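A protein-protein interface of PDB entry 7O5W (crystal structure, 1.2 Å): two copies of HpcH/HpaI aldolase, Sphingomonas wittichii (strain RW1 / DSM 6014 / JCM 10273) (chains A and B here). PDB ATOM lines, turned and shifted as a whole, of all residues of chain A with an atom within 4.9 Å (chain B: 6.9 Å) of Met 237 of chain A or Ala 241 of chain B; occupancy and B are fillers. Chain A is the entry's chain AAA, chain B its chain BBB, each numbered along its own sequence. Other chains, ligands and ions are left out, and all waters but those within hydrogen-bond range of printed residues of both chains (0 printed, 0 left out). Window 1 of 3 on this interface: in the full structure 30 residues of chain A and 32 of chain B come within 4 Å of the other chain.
Leu 31 of chain A touches Ala 242 of chain B (CG to CB, 3.97 Å). Ile 246 of chain B touches Tyr 36 of chain A (CG1 to CE1, 3.6 Å). Ala 232 of chain A touches Val 245 of chain B (N to CG1, 3.8 Å). Asp 234 of chain A touches Leu 238 of chain B (O to CD1, 3.6 Å). CE of Met 237 of chain A touches CD1 of Leu 238 of chain B (3.8 Å). Ala 241 of chain B touches Met 237 of chain A (CB to CB, 3.96 Å). SD of Met 237 of chain A touches CA of Ala 242 of chain B (3.8 Å). Met 237 of chain A touches Val 245 of chain B (SD to CG2, 3.6 Å). Leu 238 of chain A touches Met 237 of chain B (CD1 to CE, 3.9 Å). Ala 241 of chain A touches Met 237 of chain B.
Met 237 of chain A touches just these residues of chain B: Leu 238 (3.8 Å), Ala 241 (3.96 Å), Ala 242 (3.8 Å) and Val 245 (3.6 Å). Of chain A, only Met 237 comes within 4 Å of Ala 241 of chain B. Of the printed residues of chain B, Ala 241 of chain A touches Met 237. Printed residues of chain A within 4 Å of Val 245 of chain B: Ala 232 and Met 237. Leu 235 of chain A touches none of the printed residues of chain B. The nearest residue of chain A that does not touch Ala 241 of chain B is Ala 241 of chain A (4.5 Å).
Of the 13 printed residues of chain B, 6 touch a printed residue of chain A. Printed residues of chain B that touch a printed residue of chain A: Met 237, Leu 238, Ala 241, Ala 242, Val 245 and Ile 246. Hydrophobic or aromatic side chains of chain B within 4 Å of the printed part of chain A: Met 237, Leu 238, Ala 241, Ala 242, Val 245 and Ile 246. Of the 12 printed residues of chain A, 7 touch a printed residue of chain B. Hydrophobic or aromatic side chains of chain A that line the printed part of chain B: Leu 31, Tyr 36, Met 237, Leu 238 and Ala 241.
Met 237 of chain A touches Leu 238 of chain B, and with the chains exchanged Leu 238 of chain A touches Met 237 of chain B. Met 237 of chain A touches Ala 241 of chain B, and with the chains exchanged Ala 241 of chain A touches Met 237 of chain B. Positions printed for both chains: 235, 236, 237, 238, 239, 240 and 241.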
ATOM      1  N   LEU A  31      20.764 -25.788  -6.788  1.00  0.00           N
ATOM      2  CA  LEU A  31      19.988 -25.936  -8.009  1.00  0.00           C
ATOM      3  C   LEU A  31      20.166 -27.341  -8.582  1.00  0.00           C
ATOM      4  O   LEU A  31      19.180 -27.913  -9.106  1.00  0.00           O
ATOM      5  CB  LEU A  31      20.300 -24.847  -9.026  1.00  0.00           C
ATOM      6  CG  LEU A  31      19.408 -23.604  -8.916  1.00  0.00           C
ATOM      7  CD1 LEU A  31      19.334 -23.033  -7.522  1.00  0.00           C
ATOM      8  CD2 LEU A  31      19.838 -22.553  -9.890  1.00  0.00           C
ATOM      9  N   TYR A  36      16.375 -30.704 -11.957  1.00  0.00           N
ATOM     10  CA  TYR A  36      17.169 -30.471 -13.153  1.00  0.00           C
ATOM     11  C   TYR A  36      17.968 -31.742 -13.448  1.00  0.00           C
ATOM     12  O   TYR A  36      18.579 -32.291 -12.513  1.00  0.00           O
ATOM     13  CB  TYR A  36      18.148 -29.323 -12.974  1.00  0.00           C
ATOM     14  CG  TYR A  36      17.641 -27.914 -13.019  1.00  0.00           C
ATOM     15  CD1 TYR A  36      16.800 -27.483 -14.056  1.00  0.00           C
ATOM     16  CD2 TYR A  36      18.030 -26.982 -12.075  1.00  0.00           C
ATOM     17  CE1 TYR A  36      16.432 -26.145 -14.186  1.00  0.00           C
ATOM     18  CE2 TYR A  36      17.680 -25.652 -12.214  1.00  0.00           C
ATOM     19  CZ  TYR A  36      16.889 -25.237 -13.269  1.00  0.00           C
ATOM     20  OH  TYR A  36      16.597 -23.893 -13.359  1.00  0.00           O
ATOM     21  N   ALA A 232      15.946 -21.174 -15.986  1.00  0.00           N
ATOM     22  CA  ALA A 232      16.250 -19.905 -16.616  1.00  0.00           C
ATOM     23  C   ALA A 232      17.517 -19.390 -15.937  1.00  0.00           C
ATOM     24  O   ALA A 232      17.927 -19.916 -14.904  1.00  0.00           O
ATOM     25  CB  ALA A 232      15.085 -18.973 -16.456  1.00  0.00           C
ATOM     26  N   PRO A 233      18.185 -18.367 -16.473  1.00  0.00           N
ATOM     27  CA  PRO A 233      19.446 -17.955 -15.854  1.00  0.00           C
ATOM     28  C   PRO A 233      19.281 -17.586 -14.373  1.00  0.00           C
ATOM     29  O   PRO A 233      18.353 -16.819 -14.011  1.00  0.00           O
ATOM     30  CB  PRO A 233      19.856 -16.768 -16.687  1.00  0.00           C
ATOM     31  CG  PRO A 233      19.253 -17.007 -18.029  1.00  0.00           C
ATOM     32  CD  PRO A 233      17.913 -17.643 -17.720  1.00  0.00           C
ATOM     33  N   ASP A 234      20.203 -18.012 -13.561  1.00  0.00           N
ATOM     34  CA  ASP A 234      20.195 -17.673 -12.118  1.00  0.00           C
ATOM     35  C   ASP A 234      20.061 -16.178 -11.882  1.00  0.00           C
ATOM     36  O   ASP A 234      19.241 -15.803 -11.055  1.00  0.00           O
ATOM     37  CB  ASP A 234      21.411 -18.276 -11.406  1.00  0.00           C
ATOM     38  CG  ASP A 234      22.809 -17.928 -11.936  1.00  0.00           C
ATOM     39  OD1 ASP A 234      22.893 -17.194 -12.949  1.00  0.00           O
ATOM     40  OD2 ASP A 234      23.770 -18.448 -11.361  1.00  0.00           O
ATOM     41  N   LEU A 235      20.882 -15.357 -12.523  1.00  0.00           N
ATOM     42  CA  LEU A 235      20.820 -13.928 -12.200  1.00  0.00           C
ATOM     43  C   LEU A 235      19.457 -13.358 -12.538  1.00  0.00           C
ATOM     44  O   LEU A 235      18.937 -12.546 -11.778  1.00  0.00           O
ATOM     45  CB  LEU A 235      21.903 -13.200 -12.983  1.00  0.00           C
ATOM     46  CG  LEU A 235      21.882 -11.679 -12.890  1.00  0.00           C
ATOM     47  CD1 LEU A 235      22.048 -11.133 -11.503  1.00  0.00           C
ATOM     48  CD2 LEU A 235      22.971 -11.102 -13.780  1.00  0.00           C
ATOM     49  N   ALA A 236      18.892 -13.710 -13.677  1.00  0.00           N
ATOM     50  CA  ALA A 236      17.561 -13.223 -14.072  1.00  0.00           C
ATOM     51  C   ALA A 236      16.494 -13.688 -13.093  1.00  0.00           C
ATOM     52  O   ALA A 236      15.632 -12.877 -12.705  1.00  0.00           O
ATOM     53  CB  ALA A 236      17.231 -13.660 -15.468  1.00  0.00           C
ATOM     54  N   MET A 237      16.540 -14.943 -12.695  1.00  0.00           N
ATOM     55  CA  MET A 237      15.533 -15.443 -11.752  1.00  0.00           C
ATOM     56  C   MET A 237      15.669 -14.736 -10.398  1.00  0.00           C
ATOM     57  O   MET A 237      14.679 -14.349  -9.767  1.00  0.00           O
ATOM     58  CB  MET A 237      15.704 -16.937 -11.542  1.00  0.00           C
ATOM     59  CG  MET A 237      15.354 -17.778 -12.780  1.00  0.00           C
ATOM     60  SD  MET A 237      15.233 -19.556 -12.428  1.00  0.00           S
ATOM     61  CE  MET A 237      16.895 -19.920 -11.881  1.00  0.00           C
ATOM     62  N   LEU A 238      16.904 -14.536  -9.952  1.00  0.00           N
ATOM     63  CA  LEU A 238      17.139 -13.906  -8.658  1.00  0.00           C
ATOM     64  C   LEU A 238      16.712 -12.431  -8.711  1.00  0.00           C
ATOM     65  O   LEU A 238      16.065 -11.924  -7.739  1.00  0.00           O
ATOM     66  CB  LEU A 238      18.637 -14.029  -8.336  1.00  0.00           C
ATOM     67  CG  LEU A 238      19.083 -13.278  -7.077  1.00  0.00           C
ATOM     68  CD1 LEU A 238      18.314 -13.640  -5.817  1.00  0.00           C
ATOM     69  CD2 LEU A 238      20.582 -13.531  -6.858  1.00  0.00           C
ATOM     70  N   SER A 239      17.061 -11.714  -9.754  1.00  0.00           N
ATOM     71  CA  SER A 239      16.665 -10.289  -9.886  1.00  0.00           C
ATOM     72  C   SER A 239      15.150 -10.154  -9.857  1.00  0.00           C
ATOM     73  O   SER A 239      14.600  -9.274  -9.193  1.00  0.00           O
ATOM     74  CB  SER A 239      17.223  -9.731 -11.178  1.00  0.00           C
ATOM     75  OG  SER A 239      18.645  -9.771 -11.126  1.00  0.00           O
ATOM     76  N   ALA A 240      14.474 -10.990 -10.632  1.00  0.00           N
ATOM     77  CA  ALA A 240      13.014 -10.904 -10.699  1.00  0.00           C
ATOM     78  C   ALA A 240      12.441 -11.237  -9.315  1.00  0.00           C
ATOM     79  O   ALA A 240      11.437 -10.584  -8.878  1.00  0.00           O
ATOM     80  CB  ALA A 240      12.488 -11.816 -11.758  1.00  0.00           C
ATOM     81  N   ALA A 241      12.974 -12.215  -8.637  1.00  0.00           N
ATOM     82  CA  ALA A 241      12.456 -12.587  -7.312  1.00  0.00           C
ATOM     83  C   ALA A 241      12.641 -11.419  -6.351  1.00  0.00           C
ATOM     84  O   ALA A 241      11.722 -11.117  -5.556  1.00  0.00           O
ATOM     85  CB  ALA A 241      13.157 -13.807  -6.792  1.00  0.00           C
ATOM     86  N   LEU B 235      19.928 -16.735  -1.688  1.00  0.00           N
ATOM     87  CA  LEU B 235      19.861 -18.167  -1.957  1.00  0.00           C
ATOM     88  C   LEU B 235      18.420 -18.673  -1.883  1.00  0.00           C
ATOM     89  O   LEU B 235      17.997 -19.460  -2.743  1.00  0.00           O
ATOM     90  CB  LEU B 235      20.725 -18.926  -0.981  1.00  0.00           C
ATOM     91  CG  LEU B 235      20.646 -20.432  -1.057  1.00  0.00           C
ATOM     92  CD1 LEU B 235      21.069 -21.004  -2.392  1.00  0.00           C
ATOM     93  CD2 LEU B 235      21.494 -21.038   0.072  1.00  0.00           C
ATOM     94  N   ALA B 236      17.678 -18.282  -0.878  1.00  0.00           N
ATOM     95  CA  ALA B 236      16.297 -18.734  -0.711  1.00  0.00           C
ATOM     96  C   ALA B 236      15.446 -18.212  -1.884  1.00  0.00           C
ATOM     97  O   ALA B 236      14.608 -18.977  -2.412  1.00  0.00           O
ATOM     98  CB  ALA B 236      15.732 -18.255   0.605  1.00  0.00           C
ATOM     99  N   MET B 237      15.620 -16.987  -2.284  1.00  0.00           N
ATOM    100  CA  MET B 237      14.841 -16.415  -3.373  1.00  0.00           C
ATOM    101  C   MET B 237      15.161 -17.164  -4.668  1.00  0.00           C
ATOM    102  O   MET B 237      14.261 -17.481  -5.476  1.00  0.00           O
ATOM    103  CB  MET B 237      15.096 -14.929  -3.566  1.00  0.00           C
ATOM    104  CG  MET B 237      14.546 -14.070  -2.429  1.00  0.00           C
ATOM    105  SD  MET B 237      14.567 -12.295  -2.742  1.00  0.00           S
ATOM    106  CE  MET B 237      16.323 -11.973  -2.929  1.00  0.00           C
ATOM    107  N   LEU B 238      16.438 -17.412  -4.920  1.00  0.00           N
ATOM    108  CA  LEU B 238      16.867 -18.089  -6.133  1.00  0.00           C
ATOM    109  C   LEU B 238      16.390 -19.526  -6.175  1.00  0.00           C
ATOM    110  O   LEU B 238      15.914 -19.983  -7.223  1.00  0.00           O
ATOM    111  CB  LEU B 238      18.391 -17.978  -6.205  1.00  0.00           C
ATOM    112  CG  LEU B 238      19.030 -18.761  -7.360  1.00  0.00           C
ATOM    113  CD1 LEU B 238      18.496 -18.417  -8.730  1.00  0.00           C
ATOM    114  CD2 LEU B 238      20.534 -18.543  -7.309  1.00  0.00           C
ATOM    115  N   SER B 239      16.549 -20.236  -5.087  1.00  0.00           N
ATOM    116  CA  SER B 239      16.097 -21.645  -5.042  1.00  0.00           C
ATOM    117  C   SER B 239      14.607 -21.708  -5.318  1.00  0.00           C
ATOM    118  O   SER B 239      14.135 -22.565  -6.080  1.00  0.00           O
ATOM    119  CB  SER B 239      16.448 -22.289  -3.733  1.00  0.00           C
ATOM    120  OG  SER B 239      16.085 -23.663  -3.742  1.00  0.00           O
ATOM    121  N   ALA B 240      13.836 -20.881  -4.654  1.00  0.00           N
ATOM    122  CA  ALA B 240      12.377 -20.902  -4.836  1.00  0.00           C
ATOM    123  C   ALA B 240      12.034 -20.525  -6.285  1.00  0.00           C
ATOM    124  O   ALA B 240      11.109 -21.149  -6.848  1.00  0.00           O
ATOM    125  CB  ALA B 240      11.712 -19.964  -3.877  1.00  0.00           C
ATOM    126  N   ALA B 241      12.714 -19.561  -6.856  1.00  0.00           N
ATOM    127  CA  ALA B 241      12.432 -19.187  -8.227  1.00  0.00           C
ATOM    128  C   ALA B 241      12.749 -20.330  -9.171  1.00  0.00           C
ATOM    129  O   ALA B 241      11.958 -20.615 -10.092  1.00  0.00           O
ATOM    130  CB  ALA B 241      13.231 -17.966  -8.619  1.00  0.00           C
ATOM    131  N   ALA B 242      13.851 -21.011  -8.974  1.00  0.00           N
ATOM    132  CA  ALA B 242      14.215 -22.147  -9.853  1.00  0.00           C
ATOM    133  C   ALA B 242      13.217 -23.289  -9.674  1.00  0.00           C
ATOM    134  O   ALA B 242      12.804 -23.904 -10.669  1.00  0.00           O
ATOM    135  CB  ALA B 242      15.603 -22.650  -9.494  1.00  0.00           C
ATOM    136  N   ARG B 243      12.805 -23.572  -8.441  1.00  0.00           N
ATOM    137  CA  ARG B 243      11.781 -24.622  -8.249  1.00  0.00           C
ATOM    138  C   ARG B 243      10.520 -24.288  -9.040  1.00  0.00           C
ATOM    139  O   ARG B 243       9.915 -25.204  -9.633  1.00  0.00           O
ATOM    140  CB  ARG B 243      11.502 -24.756  -6.757  1.00  0.00           C
ATOM    141  CG  ARG B 243      10.615 -25.879  -6.320  1.00  0.00           C
ATOM    142  CD  ARG B 243      10.529 -25.832  -4.784  1.00  0.00           C
ATOM    143  NE  ARG B 243      11.800 -25.438  -4.114  1.00  0.00           N
ATOM    144  CZ  ARG B 243      12.072 -24.328  -3.298  1.00  0.00           C
ATOM    145  NH1 ARG B 243      11.094 -23.465  -3.055  1.00  0.00           N
ATOM    146  NH2 ARG B 243      13.288 -24.044  -2.735  1.00  0.00           N
ATOM    147  N   GLN B 244      10.123 -23.046  -9.046  1.00  0.00           N
ATOM    148  CA  GLN B 244       8.902 -22.660  -9.766  1.00  0.00           C
ATOM    149  C   GLN B 244       9.096 -22.721 -11.270  1.00  0.00           C
ATOM    150  O   GLN B 244       8.198 -23.157 -11.988  1.00  0.00           O
ATOM    151  CB  GLN B 244       8.441 -21.279  -9.320  1.00  0.00           C
ATOM    152  CG  GLN B 244       7.102 -20.914  -9.902  1.00  0.00           C
ATOM    153  CD  GLN B 244       5.999 -21.828  -9.416  1.00  0.00           C
ATOM    154  OE1 GLN B 244       5.764 -21.910  -8.204  1.00  0.00           O
ATOM    155  NE2 GLN B 244       5.362 -22.546 -10.330  1.00  0.00           N
ATOM    156  N   VAL B 245      10.254 -22.295 -11.769  1.00  0.00           N
ATOM    157  CA  VAL B 245      10.537 -22.430 -13.196  1.00  0.00           C
ATOM    158  C   VAL B 245      10.492 -23.897 -13.618  1.00  0.00           C
ATOM    159  O   VAL B 245       9.904 -24.235 -14.661  1.00  0.00           O
ATOM    160  CB  VAL B 245      11.888 -21.805 -13.554  1.00  0.00           C
ATOM    161  CG1 VAL B 245      12.412 -22.254 -14.921  1.00  0.00           C
ATOM    162  CG2 VAL B 245      11.817 -20.279 -13.483  1.00  0.00           C
ATOM    163  N   ILE B 246      11.056 -24.793 -12.832  1.00  0.00           N
ATOM    164  CA  ILE B 246      11.034 -26.233 -13.143  1.00  0.00           C
ATOM    165  C   ILE B 246       9.607 -26.755 -13.109  1.00  0.00           C
ATOM    166  O   ILE B 246       9.187 -27.505 -14.027  1.00  0.00           O
ATOM    167  CB  ILE B 246      11.907 -26.995 -12.165  1.00  0.00           C
ATOM    168  CG1 ILE B 246      13.375 -26.637 -12.376  1.00  0.00           C
ATOM    169  CG2 ILE B 246      11.663 -28.483 -12.295  1.00  0.00           C
ATOM    170  CD1 ILE B 246      14.283 -27.124 -11.192  1.00  0.00           C
ATOM    171  N   ALA B 247       8.833 -26.364 -12.125  1.00  0.00           N
ATOM    172  CA  ALA B 247       7.444 -26.849 -12.065  1.00  0.00           C
ATOM    173  C   ALA B 247       6.683 -26.358 -13.267  1.00  0.00           C
ATOM    174  O   ALA B 247       5.901 -27.124 -13.862  1.00  0.00           O
ATOM    175  CB  ALA B 247       6.796 -26.342 -10.791  1.00  0.00           C
